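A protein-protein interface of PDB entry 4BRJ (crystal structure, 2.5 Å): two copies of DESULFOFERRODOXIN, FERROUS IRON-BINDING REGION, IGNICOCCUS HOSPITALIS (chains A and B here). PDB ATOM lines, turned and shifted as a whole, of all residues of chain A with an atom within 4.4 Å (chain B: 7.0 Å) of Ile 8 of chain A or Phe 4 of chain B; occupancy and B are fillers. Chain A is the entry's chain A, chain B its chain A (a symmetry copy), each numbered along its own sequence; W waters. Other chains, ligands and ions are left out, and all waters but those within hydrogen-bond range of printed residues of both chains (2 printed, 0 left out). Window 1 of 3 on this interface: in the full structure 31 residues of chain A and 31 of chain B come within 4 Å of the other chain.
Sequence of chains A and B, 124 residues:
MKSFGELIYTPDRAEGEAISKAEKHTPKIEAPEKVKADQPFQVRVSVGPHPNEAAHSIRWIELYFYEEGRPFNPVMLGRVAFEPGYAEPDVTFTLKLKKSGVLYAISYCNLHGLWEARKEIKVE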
ATOM      1  N   PHE A   4     -26.878 -12.009  20.813  1.00  0.00           N
ATOM      2  CA  PHE A   4     -27.022 -11.389  19.492  1.00  0.00           C
ATOM      3  C   PHE A   4     -26.032 -10.245  19.260  1.00  0.00           C
ATOM      4  O   PHE A   4     -25.419 -10.149  18.200  1.00  0.00           O
ATOM      5  CB  PHE A   4     -28.464 -10.898  19.246  1.00  0.00           C
ATOM      6  CG  PHE A   4     -28.653 -10.246  17.910  1.00  0.00           C
ATOM      7  CD1 PHE A   4     -28.906 -11.012  16.775  1.00  0.00           C
ATOM      8  CD2 PHE A   4     -28.541  -8.878  17.772  1.00  0.00           C
ATOM      9  CE1 PHE A   4     -29.065 -10.420  15.528  1.00  0.00           C
ATOM     10  CE2 PHE A   4     -28.693  -8.280  16.539  1.00  0.00           C
ATOM     11  CZ  PHE A   4     -28.966  -9.055  15.410  1.00  0.00           C
ATOM     12  N   GLY A   5     -25.872  -9.383  20.257  1.00  0.00           N
ATOM     13  CA  GLY A   5     -25.006  -8.229  20.108  1.00  0.00           C
ATOM     14  C   GLY A   5     -23.539  -8.564  19.881  1.00  0.00           C
ATOM     15  O   GLY A   5     -22.827  -7.785  19.222  1.00  0.00           O
ATOM     16  N   GLU A   6     -23.090  -9.703  20.427  1.00  0.00           N
ATOM     17  CA  GLU A   6     -21.729 -10.213  20.193  1.00  0.00           C
ATOM     18  C   GLU A   6     -21.497 -10.692  18.755  1.00  0.00           C
ATOM     19  O   GLU A   6     -20.348 -10.788  18.314  1.00  0.00           O
ATOM     20  CB  GLU A   6     -21.392 -11.399  21.115  1.00  0.00           C
ATOM     21  CG  GLU A   6     -21.786 -11.274  22.571  1.00  0.00           C
ATOM     22  CD  GLU A   6     -21.508 -12.558  23.337  1.00  0.00           C
ATOM     23  OE1 GLU A   6     -20.874 -13.461  22.753  1.00  0.00           O
ATOM     24  OE2 GLU A   6     -21.916 -12.666  24.515  1.00  0.00           O
ATOM     25  N   LEU A   7     -22.572 -11.019  18.031  1.00  0.00           N
ATOM     26  CA  LEU A   7     -22.396 -11.591  16.703  1.00  0.00           C
ATOM     27  C   LEU A   7     -21.901 -10.559  15.700  1.00  0.00           C
ATOM     28  O   LEU A   7     -21.343 -10.909  14.647  1.00  0.00           O
ATOM     29  CB  LEU A   7     -23.676 -12.232  16.203  1.00  0.00           C
ATOM     30  CG  LEU A   7     -24.223 -13.367  17.059  1.00  0.00           C
ATOM     31  CD1 LEU A   7     -25.406 -13.992  16.337  1.00  0.00           C
ATOM     32  CD2 LEU A   7     -23.142 -14.402  17.387  1.00  0.00           C
ATOM     33  N   ILE A   8     -22.080  -9.290  16.049  1.00  0.00           N
ATOM     34  CA  ILE A   8     -21.833  -8.201  15.113  1.00  0.00           C
ATOM     35  C   ILE A   8     -20.353  -7.834  14.993  1.00  0.00           C
ATOM     36  O   ILE A   8     -19.701  -7.507  15.975  1.00  0.00           O
ATOM     37  CB  ILE A   8     -22.670  -6.955  15.491  1.00  0.00           C
ATOM     38  CG1 ILE A   8     -24.160  -7.312  15.523  1.00  0.00           C
ATOM     39  CG2 ILE A   8     -22.363  -5.789  14.564  1.00  0.00           C
ATOM     40  CD1 ILE A   8     -25.042  -6.233  16.120  1.00  0.00           C
ATOM     41  N   TYR A   9     -19.841  -7.884  13.771  1.00  0.00           N
ATOM     42  CA  TYR A   9     -18.472  -7.497  13.484  1.00  0.00           C
ATOM     43  C   TYR A   9     -18.237  -6.026  13.774  1.00  0.00           C
ATOM     44  O   TYR A   9     -18.694  -5.164  13.038  1.00  0.00           O
ATOM     45  CB  TYR A   9     -18.116  -7.833  12.027  1.00  0.00           C
ATOM     46  CG  TYR A   9     -18.227  -9.313  11.742  1.00  0.00           C
ATOM     47  CD1 TYR A   9     -17.141 -10.169  11.941  1.00  0.00           C
ATOM     48  CD2 TYR A   9     -19.428  -9.862  11.308  1.00  0.00           C
ATOM     49  CE1 TYR A   9     -17.253 -11.535  11.700  1.00  0.00           C
ATOM     50  CE2 TYR A   9     -19.551 -11.215  11.069  1.00  0.00           C
ATOM     51  CZ  TYR A   9     -18.464 -12.051  11.267  1.00  0.00           C
ATOM     52  OH  TYR A   9     -18.603 -13.399  11.023  1.00  0.00           O
ATOM     53  N   THR A  10     -17.508  -5.746  14.850  1.00  0.00           N
ATOM     54  CA  THR A  10     -17.159  -4.373  15.198  1.00  0.00           C
ATOM     55  C   THR A  10     -16.053  -3.886  14.275  1.00  0.00           C
ATOM     56  O   THR A  10     -15.387  -4.687  13.634  1.00  0.00           O
ATOM     57  CB  THR A  10     -16.715  -4.272  16.655  1.00  0.00           C
ATOM     58  OG1 THR A  10     -15.445  -4.920  16.812  1.00  0.00           O
ATOM     59  CG2 THR A  10     -17.747  -4.917  17.558  1.00  0.00           C
ATOM     60  N   ARG A  13     -12.388  -5.594  15.192  1.00  0.00           N
ATOM     61  CA  ARG A  13     -12.086  -6.926  14.675  1.00  0.00           C
ATOM     62  C   ARG A  13     -12.573  -7.091  13.231  1.00  0.00           C
ATOM     63  O   ARG A  13     -12.799  -8.207  12.758  1.00  0.00           O
ATOM     64  CB  ARG A  13     -12.657  -8.025  15.586  1.00  0.00           C
ATOM     65  CG  ARG A  13     -14.179  -8.164  15.582  1.00  0.00           C
ATOM     66  CD  ARG A  13     -14.593  -9.637  15.559  1.00  0.00           C
ATOM     67  NE  ARG A  13     -16.027  -9.827  15.777  1.00  0.00           N
ATOM     68  CZ  ARG A  13     -16.663 -10.978  15.574  1.00  0.00           C
ATOM     69  NH1 ARG A  13     -15.992 -12.039  15.140  1.00  0.00           N
ATOM     70  NH2 ARG A  13     -17.969 -11.067  15.801  1.00  0.00           N
ATOM     71  N   TYR A  64     -28.749   4.073  13.163  1.00  0.00           N
ATOM     72  CA  TYR A  64     -29.229   4.276  14.520  1.00  0.00           C
ATOM     73  C   TYR A  64     -28.478   5.442  15.170  1.00  0.00           C
ATOM     74  O   TYR A  64     -27.484   5.933  14.624  1.00  0.00           O
ATOM     75  CB  TYR A  64     -28.975   3.033  15.366  1.00  0.00           C
ATOM     76  CG  TYR A  64     -29.812   1.806  15.088  1.00  0.00           C
ATOM     77  CD1 TYR A  64     -31.002   1.592  15.768  1.00  0.00           C
ATOM     78  CD2 TYR A  64     -29.380   0.830  14.187  1.00  0.00           C
ATOM     79  CE1 TYR A  64     -31.768   0.453  15.556  1.00  0.00           C
ATOM     80  CE2 TYR A  64     -30.139  -0.321  13.951  1.00  0.00           C
ATOM     81  CZ  TYR A  64     -31.340  -0.505  14.639  1.00  0.00           C
ATOM     82  OH  TYR A  64     -32.102  -1.647  14.423  1.00  0.00           O
ATOM     83  N   PRO A  74     -30.840   2.767  21.639  1.00  0.00           N
ATOM     84  CA  PRO A  74     -30.721   3.926  20.750  1.00  0.00           C
ATOM     85  C   PRO A  74     -32.043   4.255  20.061  1.00  0.00           C
ATOM     86  O   PRO A  74     -33.037   3.550  20.226  1.00  0.00           O
ATOM     87  CB  PRO A  74     -29.699   3.447  19.720  1.00  0.00           C
ATOM     88  CG  PRO A  74     -30.009   2.008  19.569  1.00  0.00           C
ATOM     89  CD  PRO A  74     -30.426   1.530  20.955  1.00  0.00           C
ATOM     90  N   TYR A 104     -24.637   5.197  14.510  1.00  0.00           N
ATOM     91  CA  TYR A 104     -24.239   3.823  14.200  1.00  0.00           C
ATOM     92  C   TYR A 104     -24.787   3.392  12.832  1.00  0.00           C
ATOM     93  O   TYR A 104     -25.954   3.648  12.509  1.00  0.00           O
ATOM     94  CB  TYR A 104     -24.763   2.858  15.252  1.00  0.00           C
ATOM     95  CG  TYR A 104     -24.189   3.057  16.645  1.00  0.00           C
ATOM     96  CD1 TYR A 104     -24.799   3.930  17.551  1.00  0.00           C
ATOM     97  CD2 TYR A 104     -23.058   2.364  17.058  1.00  0.00           C
ATOM     98  CE1 TYR A 104     -24.305   4.105  18.816  1.00  0.00           C
ATOM     99  CE2 TYR A 104     -22.546   2.540  18.334  1.00  0.00           C
ATOM    100  CZ  TYR A 104     -23.173   3.413  19.205  1.00  0.00           C
ATOM    101  OH  TYR A 104     -22.689   3.595  20.466  1.00  0.00           O
ATOM    102  N   ILE A 106     -25.322  -0.006  10.457  1.00  0.00           N
ATOM    103  CA  ILE A 106     -25.269  -1.455  10.335  1.00  0.00           C
ATOM    104  C   ILE A 106     -25.557  -1.943   8.900  1.00  0.00           C
ATOM    105  O   ILE A 106     -26.646  -1.720   8.344  1.00  0.00           O
ATOM    106  CB  ILE A 106     -26.195  -2.147  11.335  1.00  0.00           C
ATOM    107  CG1 ILE A 106     -25.981  -1.585  12.749  1.00  0.00           C
ATOM    108  CG2 ILE A 106     -25.938  -3.638  11.302  1.00  0.00           C
ATOM    109  CD1 ILE A 106     -24.568  -1.820  13.299  1.00  0.00           C
ATOM    110  N   LEU A 114     -23.464  -9.139   9.793  1.00  0.00           N
ATOM    111  CA  LEU A 114     -23.719  -7.769  10.263  1.00  0.00           C
ATOM    112  C   LEU A 114     -22.453  -7.008  10.619  1.00  0.00           C
ATOM    113  O   LEU A 114     -21.659  -7.445  11.473  1.00  0.00           O
ATOM    114  CB  LEU A 114     -24.656  -7.791  11.472  1.00  0.00           C
ATOM    115  CG  LEU A 114     -26.061  -8.361  11.246  1.00  0.00           C
ATOM    116  CD1 LEU A 114     -26.734  -8.738  12.580  1.00  0.00           C
ATOM    117  CD2 LEU A 114     -26.915  -7.373  10.436  1.00  0.00           C
ATOM    118  N   GLU A 116     -20.610  -3.149  11.619  1.00  0.00           N
ATOM    119  CA  GLU A 116     -20.872  -1.929  12.395  1.00  0.00           C
ATOM    120  C   GLU A 116     -19.880  -0.785  12.188  1.00  0.00           C
ATOM    121  O   GLU A 116     -18.678  -0.992  12.117  1.00  0.00           O
ATOM    122  CB  GLU A 116     -20.935  -2.247  13.889  1.00  0.00           C
ATOM    123  CG  GLU A 116     -21.023  -0.982  14.771  1.00  0.00           C
ATOM    124  CD  GLU A 116     -20.631  -1.210  16.221  1.00  0.00           C
ATOM    125  OE1 GLU A 116     -20.059  -2.278  16.554  1.00  0.00           O
ATOM    126  OE2 GLU A 116     -20.901  -0.311  17.031  1.00  0.00           O
ATOM    127  N   LYS B   2     -19.073   3.355  23.503  1.00  0.00           N
ATOM    128  CA  LYS B   2     -19.878   2.118  23.572  1.00  0.00           C
ATOM    129  C   LYS B   2     -20.188   1.507  22.175  1.00  0.00           C
ATOM    130  O   LYS B   2     -20.455   2.236  21.227  1.00  0.00           O
ATOM    131  CB  LYS B   2     -21.203   2.386  24.293  1.00  0.00           C
ATOM    132  CG  LYS B   2     -21.350   1.682  25.639  1.00  0.00           C
ATOM    133  CD  LYS B   2     -22.548   2.214  26.422  1.00  0.00           C
ATOM    134  CE  LYS B   2     -22.450   3.719  26.648  1.00  0.00           C
ATOM    135  NZ  LYS B   2     -23.650   4.248  27.356  1.00  0.00           N
ATOM    136  N   SER B   3     -20.155   0.179  22.054  1.00  0.00           N
ATOM    137  CA  SER B   3     -20.461  -0.476  20.780  1.00  0.00           C
ATOM    138  C   SER B   3     -21.964  -0.734  20.617  1.00  0.00           C
ATOM    139  O   SER B   3     -22.688  -0.881  21.608  1.00  0.00           O
ATOM    140  CB  SER B   3     -19.682  -1.791  20.609  1.00  0.00           C
ATOM    141  OG  SER B   3     -20.420  -2.902  21.087  1.00  0.00           O
ATOM    142  N   PHE B   4     -22.416  -0.790  19.365  1.00  0.00           N
ATOM    143  CA  PHE B   4     -23.836  -0.997  19.061  1.00  0.00           C
ATOM    144  C   PHE B   4     -24.410  -2.251  19.726  1.00  0.00           C
ATOM    145  O   PHE B   4     -25.501  -2.221  20.288  1.00  0.00           O
ATOM    146  CB  PHE B   4     -24.092  -1.041  17.539  1.00  0.00           C
ATOM    147  CG  PHE B   4     -25.531  -1.264  17.184  1.00  0.00           C
ATOM    148  CD1 PHE B   4     -26.422  -0.196  17.127  1.00  0.00           C
ATOM    149  CD2 PHE B   4     -26.007  -2.536  16.943  1.00  0.00           C
ATOM    150  CE1 PHE B   4     -27.762  -0.394  16.816  1.00  0.00           C
ATOM    151  CE2 PHE B   4     -27.335  -2.743  16.636  1.00  0.00           C
ATOM    152  CZ  PHE B   4     -28.218  -1.664  16.564  1.00  0.00           C
ATOM    153  N   GLY B   5     -23.668  -3.350  19.666  1.00  0.00           N
ATOM    154  CA  GLY B   5     -24.156  -4.604  20.208  1.00  0.00           C
ATOM    155  C   GLY B   5     -24.396  -4.592  21.711  1.00  0.00           C
ATOM    156  O   GLY B   5     -25.273  -5.327  22.198  1.00  0.00           O
ATOM    157  N   GLU B   6     -23.619  -3.776  22.439  1.00  0.00           N
ATOM    158  CA  GLU B   6     -23.817  -3.572  23.883  1.00  0.00           C
ATOM    159  C   GLU B   6     -25.107  -2.815  24.221  1.00  0.00           C
ATOM    160  O   GLU B   6     -25.590  -2.894  25.355  1.00  0.00           O
ATOM    161  CB  GLU B   6     -22.659  -2.781  24.516  1.00  0.00           C
ATOM    162  CG  GLU B   6     -21.254  -3.173  24.112  1.00  0.00           C
ATOM    163  CD  GLU B   6     -20.218  -2.235  24.712  1.00  0.00           C
ATOM    164  OE1 GLU B   6     -20.606  -1.396  25.553  1.00  0.00           O
ATOM    165  OE2 GLU B   6     -19.023  -2.334  24.352  1.00  0.00           O
ATOM    166  N   LEU B   7     -25.651  -2.061  23.262  1.00  0.00           N
ATOM    167  CA  LEU B   7     -26.808  -1.231  23.570  1.00  0.00           C
ATOM    168  C   LEU B   7     -28.065  -2.062  23.781  1.00  0.00           C
ATOM    169  O   LEU B   7     -29.036  -1.603  24.403  1.00  0.00           O
ATOM    170  CB  LEU B   7     -27.044  -0.190  22.492  1.00  0.00           C
ATOM    171  CG  LEU B   7     -25.900   0.787  22.258  1.00  0.00           C
ATOM    172  CD1 LEU B   7     -26.362   1.846  21.269  1.00  0.00           C
ATOM    173  CD2 LEU B   7     -25.404   1.406  23.568  1.00  0.00           C
ATOM    174  N   ILE B   8     -28.025  -3.294  23.286  1.00  0.00           N
ATOM    175  CA  ILE B   8     -29.214  -4.135  23.241  1.00  0.00           C
ATOM    176  C   ILE B   8     -29.525  -4.810  24.578  1.00  0.00           C
ATOM    177  O   ILE B   8     -28.701  -5.526  25.132  1.00  0.00           O
ATOM    178  CB  ILE B   8     -29.096  -5.192  22.116  1.00  0.00           C
ATOM    179  CG1 ILE B   8     -28.873  -4.501  20.767  1.00  0.00           C
ATOM    180  CG2 ILE B   8     -30.300  -6.121  22.111  1.00  0.00           C
ATOM    181  CD1 ILE B   8     -28.498  -5.446  19.643  1.00  0.00           C
ATOM    182  N   ASN B  73     -22.038 -15.542  10.384  1.00  0.00           N
ATOM    183  CA  ASN B  73     -23.338 -15.557  11.048  1.00  0.00           C
ATOM    184  C   ASN B  73     -23.668 -14.136  11.499  1.00  0.00           C
ATOM    185  O   ASN B  73     -22.762 -13.289  11.569  1.00  0.00           O
ATOM    186  CB  ASN B  73     -23.310 -16.513  12.244  1.00  0.00           C
ATOM    187  CG  ASN B  73     -23.901 -17.884  11.925  1.00  0.00           C
ATOM    188  OD1 ASN B  73     -25.054 -17.993  11.496  1.00  0.00           O
ATOM    189  ND2 ASN B  73     -23.110 -18.945  12.150  1.00  0.00           N
ATOM    190  N   PRO B  74     -24.959 -13.851  11.775  1.00  0.00           N
ATOM    191  CA  PRO B  74     -26.111 -14.737  11.589  1.00  0.00           C
ATOM    192  C   PRO B  74     -26.766 -14.546  10.223  1.00  0.00           C
ATOM    193  O   PRO B  74     -26.363 -13.685   9.441  1.00  0.00           O
ATOM    194  CB  PRO B  74     -27.062 -14.278  12.693  1.00  0.00           C
ATOM    195  CG  PRO B  74     -26.833 -12.818  12.759  1.00  0.00           C
ATOM    196  CD  PRO B  74     -25.347 -12.621  12.486  1.00  0.00           C
ATOM    197  N   LEU B 114     -34.015  -1.502  21.874  1.00  0.00           N
ATOM    198  CA  LEU B 114     -33.878  -2.841  21.279  1.00  0.00           C
ATOM    199  C   LEU B 114     -33.809  -3.954  22.313  1.00  0.00           C
ATOM    200  O   LEU B 114     -32.932  -3.958  23.197  1.00  0.00           O
ATOM    201  CB  LEU B 114     -32.638  -2.899  20.387  1.00  0.00           C
ATOM    202  CG  LEU B 114     -32.618  -1.965  19.172  1.00  0.00           C
ATOM    203  CD1 LEU B 114     -31.189  -1.786  18.626  1.00  0.00           C
ATOM    204  CD2 LEU B 114     -33.583  -2.473  18.090  1.00  0.00           C
HETATM  205  O   HOH W   1     -22.678 -10.521  12.067  1.00  0.00           O
HETATM  206  O   HOH W   2     -21.469  -4.038  18.071  1.00  0.00           O
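Among the printed residues, pairs that only touch across the chains: Tyr 64 of chain A with Phe 4 of chain B, Tyr 104 of chain A with Phe 4 of chain B, Gly 5 of chain A with Gly 5 of chain B, Glu 116 of chain A with Ser 3 of chain B, Tyr 64 of chain A with Leu 114 of chain B, Tyr 9 of chain A with Asn 73 of chain B, Ile 8 of chain A with Phe 4 of chain B, Phe 4 of chain A with Ile 8 of chain B, Tyr 104 of chain A with Leu 7 of chain B and Ile 106 of chain A with Phe 4 of chain B.
Glu 6 of chain A touches none of the printed residues of chain B. Of the printed residues of chain B, Ile 8 of chain A touches Phe 4 (3.9 Å). Printed residues of chain B within 4 Å of Tyr 104 of chain A: Lys 2 (2.7 Å), Phe 4 (3.5 Å) and Leu 7 (3.9 Å). Of the printed residues of chain A, Ser 3 of chain B touches Glu 116. Printed residues of chain A within 4 Å of Phe 4 of chain B: Ile 8, Tyr 64, Tyr 104, Ile 106 and Glu 116.
Phe 4 of chain A touches Ile 8 of chain B, and with the chains exchanged Ile 8 of chain A touches Phe 4 of chain B. Gly 5 of chain A touches its own counterpart, Gly 5 of chain B.
The backbone NH (N) of Phe 4 of chain B is in hydrogen-bond range of the side-chain carboxylate (OE2) of Glu 116 of chain A (2.8 Å). O of Lys 2 of chain B sits at hydrogen-bond distance from OH of Tyr 104 of chain A (2.7 Å).
Of the 14 printed residues of chain A, 8 touch a printed residue of chain B. Printed residues of chain A that touch a printed residue of chain B: Phe 4, Gly 5, Ile 8, Tyr 9, Tyr 64, Tyr 104, Ile 106 and Glu 116. Hydrophobic or aromatic side chains of chain A within 4 Å of the printed part of chain B: Phe 4, Ile 8, Tyr 9, Tyr 64, Tyr 104 and Ile 106. Along chain A the printed residues that touch a printed residue of chain B span positions 4 to 116. Along chain B the printed residues that touch a printed residue of chain A span positions 2 to 114. Among the printed residues, 12 pairs touch across the chains.
Water W2 lies within hydrogen-bond range of the side-chain carboxylate of Glu 116 of chain A (2.7 Å), the backbone NH of Gly 5 of chain B (2.8 Å) and the side-chain hydroxyl of Ser 3 of chain B (3.4 Å). Water W1 lies within hydrogen-bond range of N of Leu 114 of chain A (2.8 Å), O of Asn 73 of chain B (2.8 Å) and O of Leu 7 of chain A (2.9 Å).
N of Glu 116 of chain A is in hydrogen-bond range of O of Tyr 9 of chain A, at 3.1 Å. The backbone NH (N) of Tyr 9 of chain A lies within hydrogen-bond range of the backbone carbonyl oxygen (O) of Leu 114 of chain A (3.0 Å). The backbone carbonyl oxygen (O) of Tyr 104 of chain A is in hydrogen-bond range of the backbone NH (N) of Tyr 64 of chain A (2.9 Å).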
